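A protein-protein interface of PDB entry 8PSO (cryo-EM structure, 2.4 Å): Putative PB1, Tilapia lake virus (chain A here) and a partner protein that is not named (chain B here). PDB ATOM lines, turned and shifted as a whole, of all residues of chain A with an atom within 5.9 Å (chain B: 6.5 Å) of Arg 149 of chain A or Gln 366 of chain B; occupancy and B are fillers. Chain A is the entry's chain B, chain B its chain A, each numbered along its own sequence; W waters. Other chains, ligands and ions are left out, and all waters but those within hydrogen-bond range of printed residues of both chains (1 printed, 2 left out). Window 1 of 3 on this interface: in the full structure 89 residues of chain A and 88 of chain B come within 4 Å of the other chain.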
ATOM      1  N   CYS A   9      23.924   9.710 -14.812  1.00  0.00           N
ATOM      2  CA  CYS A   9      23.902   8.256 -14.735  1.00  0.00           C
ATOM      3  C   CYS A   9      23.385   7.699 -16.052  1.00  0.00           C
ATOM      4  O   CYS A   9      22.323   8.112 -16.527  1.00  0.00           O
ATOM      5  CB  CYS A   9      23.024   7.774 -13.576  1.00  0.00           C
ATOM      6  SG  CYS A   9      22.960   5.977 -13.395  1.00  0.00           S
ATOM      7  N   LYS A  10      24.135   6.765 -16.634  1.00  0.00           N
ATOM      8  CA  LYS A  10      23.736   6.116 -17.875  1.00  0.00           C
ATOM      9  C   LYS A  10      22.909   4.857 -17.653  1.00  0.00           C
ATOM     10  O   LYS A  10      22.418   4.281 -18.629  1.00  0.00           O
ATOM     11  CB  LYS A  10      24.975   5.767 -18.706  1.00  0.00           C
ATOM     12  CG  LYS A  10      25.559   6.945 -19.470  1.00  0.00           C
ATOM     13  CD  LYS A  10      26.017   6.535 -20.861  1.00  0.00           C
ATOM     14  CE  LYS A  10      26.303   7.738 -21.753  1.00  0.00           C
ATOM     15  NZ  LYS A  10      26.418   9.018 -21.000  1.00  0.00           N
ATOM     16  N   GLY A  11      22.735   4.423 -16.407  1.00  0.00           N
ATOM     17  CA  GLY A  11      21.985   3.215 -16.121  1.00  0.00           C
ATOM     18  C   GLY A  11      22.634   1.957 -16.661  1.00  0.00           C
ATOM     19  O   GLY A  11      21.962   1.118 -17.269  1.00  0.00           O
ATOM     20  N   ASN A  12      23.940   1.811 -16.443  1.00  0.00           N
ATOM     21  CA  ASN A  12      24.694   0.654 -16.904  1.00  0.00           C
ATOM     22  C   ASN A  12      24.873  -0.406 -15.823  1.00  0.00           C
ATOM     23  O   ASN A  12      25.640  -1.352 -16.022  1.00  0.00           O
ATOM     24  CB  ASN A  12      26.068   1.092 -17.419  1.00  0.00           C
ATOM     25  CG  ASN A  12      25.994   1.803 -18.754  1.00  0.00           C
ATOM     26  OD1 ASN A  12      25.016   1.670 -19.490  1.00  0.00           O
ATOM     27  ND2 ASN A  12      27.031   2.566 -19.074  1.00  0.00           N
ATOM     28  N   LEU A  13      24.181  -0.277 -14.689  1.00  0.00           N
ATOM     29  CA  LEU A  13      24.398  -1.192 -13.575  1.00  0.00           C
ATOM     30  C   LEU A  13      23.888  -2.602 -13.845  1.00  0.00           C
ATOM     31  O   LEU A  13      24.237  -3.518 -13.093  1.00  0.00           O
ATOM     32  CB  LEU A  13      23.739  -0.642 -12.308  1.00  0.00           C
ATOM     33  CG  LEU A  13      24.272   0.706 -11.815  1.00  0.00           C
ATOM     34  CD1 LEU A  13      23.597   1.100 -10.514  1.00  0.00           C
ATOM     35  CD2 LEU A  13      25.784   0.672 -11.642  1.00  0.00           C
ATOM     36  N   LEU A  14      23.082  -2.803 -14.881  1.00  0.00           N
ATOM     37  CA  LEU A  14      22.613  -4.126 -15.266  1.00  0.00           C
ATOM     38  C   LEU A  14      23.268  -4.552 -16.573  1.00  0.00           C
ATOM     39  O   LEU A  14      23.844  -3.740 -17.302  1.00  0.00           O
ATOM     40  CB  LEU A  14      21.088  -4.153 -15.418  1.00  0.00           C
ATOM     41  CG  LEU A  14      20.251  -3.764 -14.196  1.00  0.00           C
ATOM     42  CD1 LEU A  14      18.780  -4.036 -14.465  1.00  0.00           C
ATOM     43  CD2 LEU A  14      20.710  -4.507 -12.950  1.00  0.00           C
ATOM     44  N   SER A  15      23.174  -5.847 -16.859  1.00  0.00           N
ATOM     45  CA  SER A  15      23.704  -6.375 -18.105  1.00  0.00           C
ATOM     46  C   SER A  15      22.878  -5.878 -19.288  1.00  0.00           C
ATOM     47  O   SER A  15      21.749  -5.404 -19.140  1.00  0.00           O
ATOM     48  CB  SER A  15      23.706  -7.904 -18.084  1.00  0.00           C
ATOM     49  OG  SER A  15      24.703  -8.402 -17.212  1.00  0.00           O
ATOM     50  N   GLY A  16      23.462  -5.990 -20.476  1.00  0.00           N
ATOM     51  CA  GLY A  16      22.785  -5.612 -21.692  1.00  0.00           C
ATOM     52  C   GLY A  16      21.734  -6.630 -22.083  1.00  0.00           C
ATOM     53  O   GLY A  16      21.625  -7.705 -21.487  1.00  0.00           O
ATOM     54  N   PRO A  17      20.938  -6.309 -23.100  1.00  0.00           N
ATOM     55  CA  PRO A  17      19.889  -7.239 -23.527  1.00  0.00           C
ATOM     56  C   PRO A  17      20.463  -8.453 -24.238  1.00  0.00           C
ATOM     57  O   PRO A  17      21.558  -8.417 -24.801  1.00  0.00           O
ATOM     58  CB  PRO A  17      19.026  -6.398 -24.474  1.00  0.00           C
ATOM     59  CG  PRO A  17      19.869  -5.240 -24.886  1.00  0.00           C
ATOM     60  CD  PRO A  17      21.058  -5.138 -23.982  1.00  0.00           C
ATOM     61  N   GLN A 147      23.744  -7.957 -25.924  1.00  0.00           N
ATOM     62  CA  GLN A 147      24.342  -7.390 -24.717  1.00  0.00           C
ATOM     63  C   GLN A 147      24.801  -5.952 -24.938  1.00  0.00           C
ATOM     64  O   GLN A 147      25.708  -5.467 -24.256  1.00  0.00           O
ATOM     65  CB  GLN A 147      25.509  -8.248 -24.221  1.00  0.00           C
ATOM     66  CG  GLN A 147      25.121  -9.672 -23.867  1.00  0.00           C
ATOM     67  CD  GLN A 147      25.030  -9.893 -22.373  1.00  0.00           C
ATOM     68  OE1 GLN A 147      26.000 -10.301 -21.735  1.00  0.00           O
ATOM     69  NE2 GLN A 147      23.861  -9.625 -21.804  1.00  0.00           N
ATOM     70  N   GLU A 148      24.182  -5.260 -25.889  1.00  0.00           N
ATOM     71  CA  GLU A 148      24.479  -3.859 -26.165  1.00  0.00           C
ATOM     72  C   GLU A 148      23.497  -3.001 -25.375  1.00  0.00           C
ATOM     73  O   GLU A 148      22.311  -2.934 -25.713  1.00  0.00           O
ATOM     74  CB  GLU A 148      24.384  -3.569 -27.661  1.00  0.00           C
ATOM     75  CG  GLU A 148      25.708  -3.208 -28.306  1.00  0.00           C
ATOM     76  CD  GLU A 148      25.540  -2.681 -29.716  1.00  0.00           C
ATOM     77  OE1 GLU A 148      24.895  -3.369 -30.534  1.00  0.00           O
ATOM     78  OE2 GLU A 148      26.048  -1.578 -30.005  1.00  0.00           O
ATOM     79  N   ARG A 149      23.991  -2.352 -24.325  1.00  0.00           N
ATOM     80  CA  ARG A 149      23.127  -1.549 -23.470  1.00  0.00           C
ATOM     81  C   ARG A 149      22.476  -0.432 -24.275  1.00  0.00           C
ATOM     82  O   ARG A 149      23.135   0.246 -25.068  1.00  0.00           O
ATOM     83  CB  ARG A 149      23.931  -0.968 -22.307  1.00  0.00           C
ATOM     84  CG  ARG A 149      24.566  -2.018 -21.411  1.00  0.00           C
ATOM     85  CD  ARG A 149      24.778  -1.490 -20.002  1.00  0.00           C
ATOM     86  NE  ARG A 149      25.358  -2.494 -19.119  1.00  0.00           N
ATOM     87  CZ  ARG A 149      26.652  -2.776 -19.047  1.00  0.00           C
ATOM     88  NH1 ARG A 149      27.542  -2.143 -19.793  1.00  0.00           N
ATOM     89  NH2 ARG A 149      27.064  -3.720 -18.205  1.00  0.00           N
ATOM     90  N   GLY A 150      21.177  -0.239 -24.063  1.00  0.00           N
ATOM     91  CA  GLY A 150      20.425   0.763 -24.786  1.00  0.00           C
ATOM     92  C   GLY A 150      19.903   0.326 -26.135  1.00  0.00           C
ATOM     93  O   GLY A 150      19.378   1.165 -26.876  1.00  0.00           O
ATOM     94  N   LYS A 151      20.024  -0.955 -26.478  1.00  0.00           N
ATOM     95  CA  LYS A 151      19.540  -1.495 -27.749  1.00  0.00           C
ATOM     96  C   LYS A 151      18.645  -2.688 -27.451  1.00  0.00           C
ATOM     97  O   LYS A 151      19.071  -3.845 -27.575  1.00  0.00           O
ATOM     98  CB  LYS A 151      20.701  -1.891 -28.663  1.00  0.00           C
ATOM     99  CG  LYS A 151      21.668  -0.760 -28.993  1.00  0.00           C
ATOM    100  CD  LYS A 151      21.028   0.293 -29.889  1.00  0.00           C
ATOM    101  CE  LYS A 151      21.177  -0.046 -31.367  1.00  0.00           C
ATOM    102  NZ  LYS A 151      21.759   1.085 -32.141  1.00  0.00           N
ATOM    103  N   ALA A 348      29.377   0.399 -14.505  1.00  0.00           N
ATOM    104  CA  ALA A 348      28.605  -0.780 -14.865  1.00  0.00           C
ATOM    105  C   ALA A 348      28.713  -1.832 -13.772  1.00  0.00           C
ATOM    106  O   ALA A 348      29.744  -1.958 -13.107  1.00  0.00           O
ATOM    107  CB  ALA A 348      29.081  -1.367 -16.198  1.00  0.00           C
ATOM    108  N   GLY A 349      27.632  -2.588 -13.593  1.00  0.00           N
ATOM    109  CA  GLY A 349      27.623  -3.661 -12.623  1.00  0.00           C
ATOM    110  C   GLY A 349      28.354  -4.891 -13.119  1.00  0.00           C
ATOM    111  O   GLY A 349      28.649  -5.046 -14.303  1.00  0.00           O
ATOM    112  N   ARG B 359      15.827  -5.151 -21.367  1.00  0.00           N
ATOM    113  CA  ARG B 359      16.493  -4.033 -20.697  1.00  0.00           C
ATOM    114  C   ARG B 359      16.196  -2.706 -21.395  1.00  0.00           C
ATOM    115  O   ARG B 359      17.087  -1.884 -21.618  1.00  0.00           O
ATOM    116  CB  ARG B 359      18.001  -4.274 -20.609  1.00  0.00           C
ATOM    117  CG  ARG B 359      18.398  -5.565 -19.901  1.00  0.00           C
ATOM    118  CD  ARG B 359      18.423  -5.402 -18.388  1.00  0.00           C
ATOM    119  NE  ARG B 359      18.066  -6.636 -17.697  1.00  0.00           N
ATOM    120  CZ  ARG B 359      18.916  -7.613 -17.412  1.00  0.00           C
ATOM    121  NH1 ARG B 359      20.197  -7.535 -17.733  1.00  0.00           N
ATOM    122  NH2 ARG B 359      18.470  -8.699 -16.788  1.00  0.00           N
ATOM    123  N   SER B 361      14.691  -0.328 -20.128  1.00  0.00           N
ATOM    124  CA  SER B 361      14.964   0.724 -19.157  1.00  0.00           C
ATOM    125  C   SER B 361      16.330   1.351 -19.389  1.00  0.00           C
ATOM    126  O   SER B 361      16.521   2.532 -19.096  1.00  0.00           O
ATOM    127  CB  SER B 361      14.874   0.164 -17.738  1.00  0.00           C
ATOM    128  OG  SER B 361      15.873  -0.813 -17.513  1.00  0.00           O
ATOM    129  N   GLN B 362      17.288   0.587 -19.919  1.00  0.00           N
ATOM    130  CA  GLN B 362      18.594   1.160 -20.232  1.00  0.00           C
ATOM    131  C   GLN B 362      18.489   2.206 -21.336  1.00  0.00           C
ATOM    132  O   GLN B 362      19.113   3.271 -21.251  1.00  0.00           O
ATOM    133  CB  GLN B 362      19.571   0.055 -20.633  1.00  0.00           C
ATOM    134  CG  GLN B 362      20.364  -0.511 -19.469  1.00  0.00           C
ATOM    135  CD  GLN B 362      20.842  -1.927 -19.714  1.00  0.00           C
ATOM    136  OE1 GLN B 362      20.811  -2.419 -20.842  1.00  0.00           O
ATOM    137  NE2 GLN B 362      21.286  -2.592 -18.657  1.00  0.00           N
ATOM    138  N   ALA B 363      17.711   1.920 -22.382  1.00  0.00           N
ATOM    139  CA  ALA B 363      17.502   2.910 -23.433  1.00  0.00           C
ATOM    140  C   ALA B 363      16.817   4.153 -22.881  1.00  0.00           C
ATOM    141  O   ALA B 363      17.215   5.287 -23.190  1.00  0.00           O
ATOM    142  CB  ALA B 363      16.678   2.303 -24.568  1.00  0.00           C
ATOM    143  N   VAL B 364      15.787   3.959 -22.053  1.00  0.00           N
ATOM    144  CA  VAL B 364      15.103   5.107 -21.463  1.00  0.00           C
ATOM    145  C   VAL B 364      16.071   5.920 -20.611  1.00  0.00           C
ATOM    146  O   VAL B 364      16.055   7.155 -20.635  1.00  0.00           O
ATOM    147  CB  VAL B 364      13.879   4.648 -20.648  1.00  0.00           C
ATOM    148  CG1 VAL B 364      13.160   5.850 -20.052  1.00  0.00           C
ATOM    149  CG2 VAL B 364      12.929   3.844 -21.519  1.00  0.00           C
ATOM    150  N   ALA B 365      16.925   5.242 -19.843  1.00  0.00           N
ATOM    151  CA  ALA B 365      17.873   5.934 -18.976  1.00  0.00           C
ATOM    152  C   ALA B 365      18.892   6.725 -19.784  1.00  0.00           C
ATOM    153  O   ALA B 365      19.244   7.849 -19.414  1.00  0.00           O
ATOM    154  CB  ALA B 365      18.574   4.928 -18.066  1.00  0.00           C
ATOM    155  N   GLN B 366      19.394   6.151 -20.879  1.00  0.00           N
ATOM    156  CA  GLN B 366      20.339   6.885 -21.716  1.00  0.00           C
ATOM    157  C   GLN B 366      19.687   8.123 -22.319  1.00  0.00           C
ATOM    158  O   GLN B 366      20.279   9.215 -22.323  1.00  0.00           O
ATOM    159  CB  GLN B 366      20.882   5.974 -22.817  1.00  0.00           C
ATOM    160  CG  GLN B 366      22.121   5.191 -22.416  1.00  0.00           C
ATOM    161  CD  GLN B 366      22.303   3.927 -23.233  1.00  0.00           C
ATOM    162  OE1 GLN B 366      21.941   3.875 -24.408  1.00  0.00           O
ATOM    163  NE2 GLN B 366      22.863   2.897 -22.612  1.00  0.00           N
ATOM    164  N   HIS B 367      18.459   7.980 -22.821  1.00  0.00           N
ATOM    165  CA  HIS B 367      17.779   9.136 -23.392  1.00  0.00           C
ATOM    166  C   HIS B 367      17.509  10.193 -22.327  1.00  0.00           C
ATOM    167  O   HIS B 367      17.620  11.393 -22.594  1.00  0.00           O
ATOM    168  CB  HIS B 367      16.479   8.714 -24.072  1.00  0.00           C
ATOM    169  CG  HIS B 367      15.997   9.697 -25.094  1.00  0.00           C
ATOM    170  ND1 HIS B 367      16.808  10.181 -26.098  1.00  0.00           N
ATOM    171  CD2 HIS B 367      14.793  10.293 -25.262  1.00  0.00           C
ATOM    172  CE1 HIS B 367      16.123  11.029 -26.843  1.00  0.00           C
ATOM    173  NE2 HIS B 367      14.898  11.115 -26.358  1.00  0.00           N
ATOM    174  N   PHE B 368      17.157   9.768 -21.112  1.00  0.00           N
ATOM    175  CA  PHE B 368      16.908  10.726 -20.040  1.00  0.00           C
ATOM    176  C   PHE B 368      18.190  11.419 -19.598  1.00  0.00           C
ATOM    177  O   PHE B 368      18.154  12.591 -19.218  1.00  0.00           O
ATOM    178  CB  PHE B 368      16.245  10.028 -18.854  1.00  0.00           C
ATOM    179  CG  PHE B 368      15.719  10.974 -17.811  1.00  0.00           C
ATOM    180  CD1 PHE B 368      14.901  12.033 -18.164  1.00  0.00           C
ATOM    181  CD2 PHE B 368      16.037  10.799 -16.477  1.00  0.00           C
ATOM    182  CE1 PHE B 368      14.418  12.903 -17.208  1.00  0.00           C
ATOM    183  CE2 PHE B 368      15.555  11.663 -15.517  1.00  0.00           C
ATOM    184  CZ  PHE B 368      14.744  12.716 -15.883  1.00  0.00           C
ATOM    185  N   ASN B 369      19.322  10.715 -19.624  1.00  0.00           N
ATOM    186  CA  ASN B 369      20.601  11.364 -19.357  1.00  0.00           C
ATOM    187  C   ASN B 369      20.875  12.451 -20.389  1.00  0.00           C
ATOM    188  O   ASN B 369      21.224  13.589 -20.040  1.00  0.00           O
ATOM    189  CB  ASN B 369      21.717  10.319 -19.353  1.00  0.00           C
ATOM    190  CG  ASN B 369      23.082  10.917 -19.087  1.00  0.00           C
ATOM    191  OD1 ASN B 369      23.950  10.918 -19.958  1.00  0.00           O
ATOM    192  ND2 ASN B 369      23.279  11.430 -17.879  1.00  0.00           N
ATOM    193  N   ARG B 370      20.693  12.123 -21.671  1.00  0.00           N
ATOM    194  CA  ARG B 370      20.836  13.137 -22.714  1.00  0.00           C
ATOM    195  C   ARG B 370      19.906  14.316 -22.450  1.00  0.00           C
ATOM    196  O   ARG B 370      20.311  15.480 -22.553  1.00  0.00           O
ATOM    197  CB  ARG B 370      20.546  12.529 -24.087  1.00  0.00           C
ATOM    198  CG  ARG B 370      21.680  11.702 -24.661  1.00  0.00           C
ATOM    199  CD  ARG B 370      21.440  11.390 -26.128  1.00  0.00           C
ATOM    200  NE  ARG B 370      20.427  10.357 -26.309  1.00  0.00           N
ATOM    201  CZ  ARG B 370      20.663   9.053 -26.272  1.00  0.00           C
ATOM    202  NH1 ARG B 370      21.881   8.575 -26.071  1.00  0.00           N
ATOM    203  NH2 ARG B 370      19.653   8.207 -26.440  1.00  0.00           N
ATOM    204  N   HIS B 371      18.652  14.026 -22.104  1.00  0.00           N
ATOM    205  CA  HIS B 371      17.671  15.074 -21.841  1.00  0.00           C
ATOM    206  C   HIS B 371      18.135  15.983 -20.708  1.00  0.00           C
ATOM    207  O   HIS B 371      18.089  17.213 -20.822  1.00  0.00           O
ATOM    208  CB  HIS B 371      16.325  14.422 -21.508  1.00  0.00           C
ATOM    209  CG  HIS B 371      15.211  15.390 -21.247  1.00  0.00           C
ATOM    210  ND1 HIS B 371      13.912  14.980 -21.041  1.00  0.00           N
ATOM    211  CD2 HIS B 371      15.195  16.742 -21.166  1.00  0.00           C
ATOM    212  CE1 HIS B 371      13.145  16.036 -20.839  1.00  0.00           C
ATOM    213  NE2 HIS B 371      13.899  17.117 -20.909  1.00  0.00           N
HETATM  214  O   HOH W   1      23.563   9.426 -22.461  1.00  0.00           O
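The side-chain amino group (NZ) of Lys 10 of chain A sits at hydrogen-bond distance from the side-chain amide oxygen (OD1) of Asn 369 of chain B (3.3 Å).
The side-chain amide nitrogen (NE2) of Gln 362 of chain B lies within hydrogen-bond range of the backbone carbonyl oxygen (O) of Leu 14 of chain A (3.1 Å).
NE2 of Gln 362 of chain B sits at hydrogen-bond distance from O of Ser 15 of chain A, 2.9 Å away.
NH1 of Arg 359 of chain B sits at hydrogen-bond distance from O of Ser 15 of chain A, 3.0 Å away.
Water W1 lies within hydrogen-bond range of the side-chain amide oxygen (OD1) of Asn 369 of chain B (2.9 Å), the side-chain amino group (NZ) of Lys 10 of chain A (3.2 Å) and the backbone carbonyl oxygen (O) of Gln 366 of chain B (3.3 Å).
Printed residues of chain B within 4 Å of Cys 9 of chain A: Asn 369 (3.6 Å).
Printed residues of chain B within 4 Å of Lys 10 of chain A: Ala 365 (3.9 Å), Gln 366 (3.9 Å) and Asn 369 (3.3 Å).
Of the printed residues of chain B, Gly 11 of chain A touches Gln 362 (3.2 Å).
Printed residues of chain B within 4 Å of Ser 15 of chain A: Arg 359 (3.0 Å) and Gln 362 (2.9 Å).
Arg 149 of chain A touches just these residues of chain B: Gln 362 (3.6 Å) and Gln 366 (3.6 Å).
Of the printed residues of chain A, Ala 363 of chain B touches Gly 150.
Printed residues of chain A within 4 Å of Gln 366 of chain B: Lys 10 (3.9 Å), Asn 12 (3.99 Å), Arg 149 (3.6 Å) and Gly 150 (3.5 Å).
The nearest printed residue of chain A that does not touch Gln 366 of chain B is Lys 151 of chain A (5.6 Å).
The backbone NH (N) of Gly 349 of chain A is in hydrogen-bond range of the backbone carbonyl oxygen (O) of Asn 12 of chain A.
The side-chain sulfur (SG) of Cys 9 of chain A sits close to the backbone NH (N) of Gly 11 of chain A, 3.4 Å away.
The guanidinium group of Arg 149 of chain A sits at hydrogen-bond distance from the backbone carbonyl oxygen of Leu 14 of chain A.
NE of Arg 149 of chain A lies within hydrogen-bond range of O of Asn 12 of chain A, 3.3 Å away.
The backbone carbonyl oxygen of Gly 16 of chain A sits at hydrogen-bond distance from the side-chain amide nitrogen of Gln 147 of chain A, 3.0 Å away.
Hydrophobic or aromatic side chains of chain A that line the printed part of chain B: Leu 14.
Printed residues of chain B that touch a printed residue of chain A: Arg 359, Gln 362, Ala 363, Ala 365, Gln 366 and Asn 369.
Hydrophobic or aromatic side chains of chain B within 4 Å of the printed part of chain A: Ala 363 and Ala 365.
Among the printed residues, 15 pairs touch across the chains.
Among the printed residues, pairs that only touch across the chains: Cys 9 of chain A with Asn 369 of chain B, Lys 10 of chain A with Ala 365 of chain B, Lys 10 of chain A with Gln 366 of chain B, Gly 11 of chain A with Gln 362 of chain B, Asn 12 of chain A with Gln 366 of chain B, Gly 16 of chain A with Gln 362 of chain B, Arg 149 of chain A with Gln 362 of chain B, Arg 149 of chain A with Gln 366 of chain B, Gly 150 of chain A with Gln 362 of chain B, Gly 150 of chain A with Ala 363 of chain B and Gly 150 of chain A with Gln 366 of chain B.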
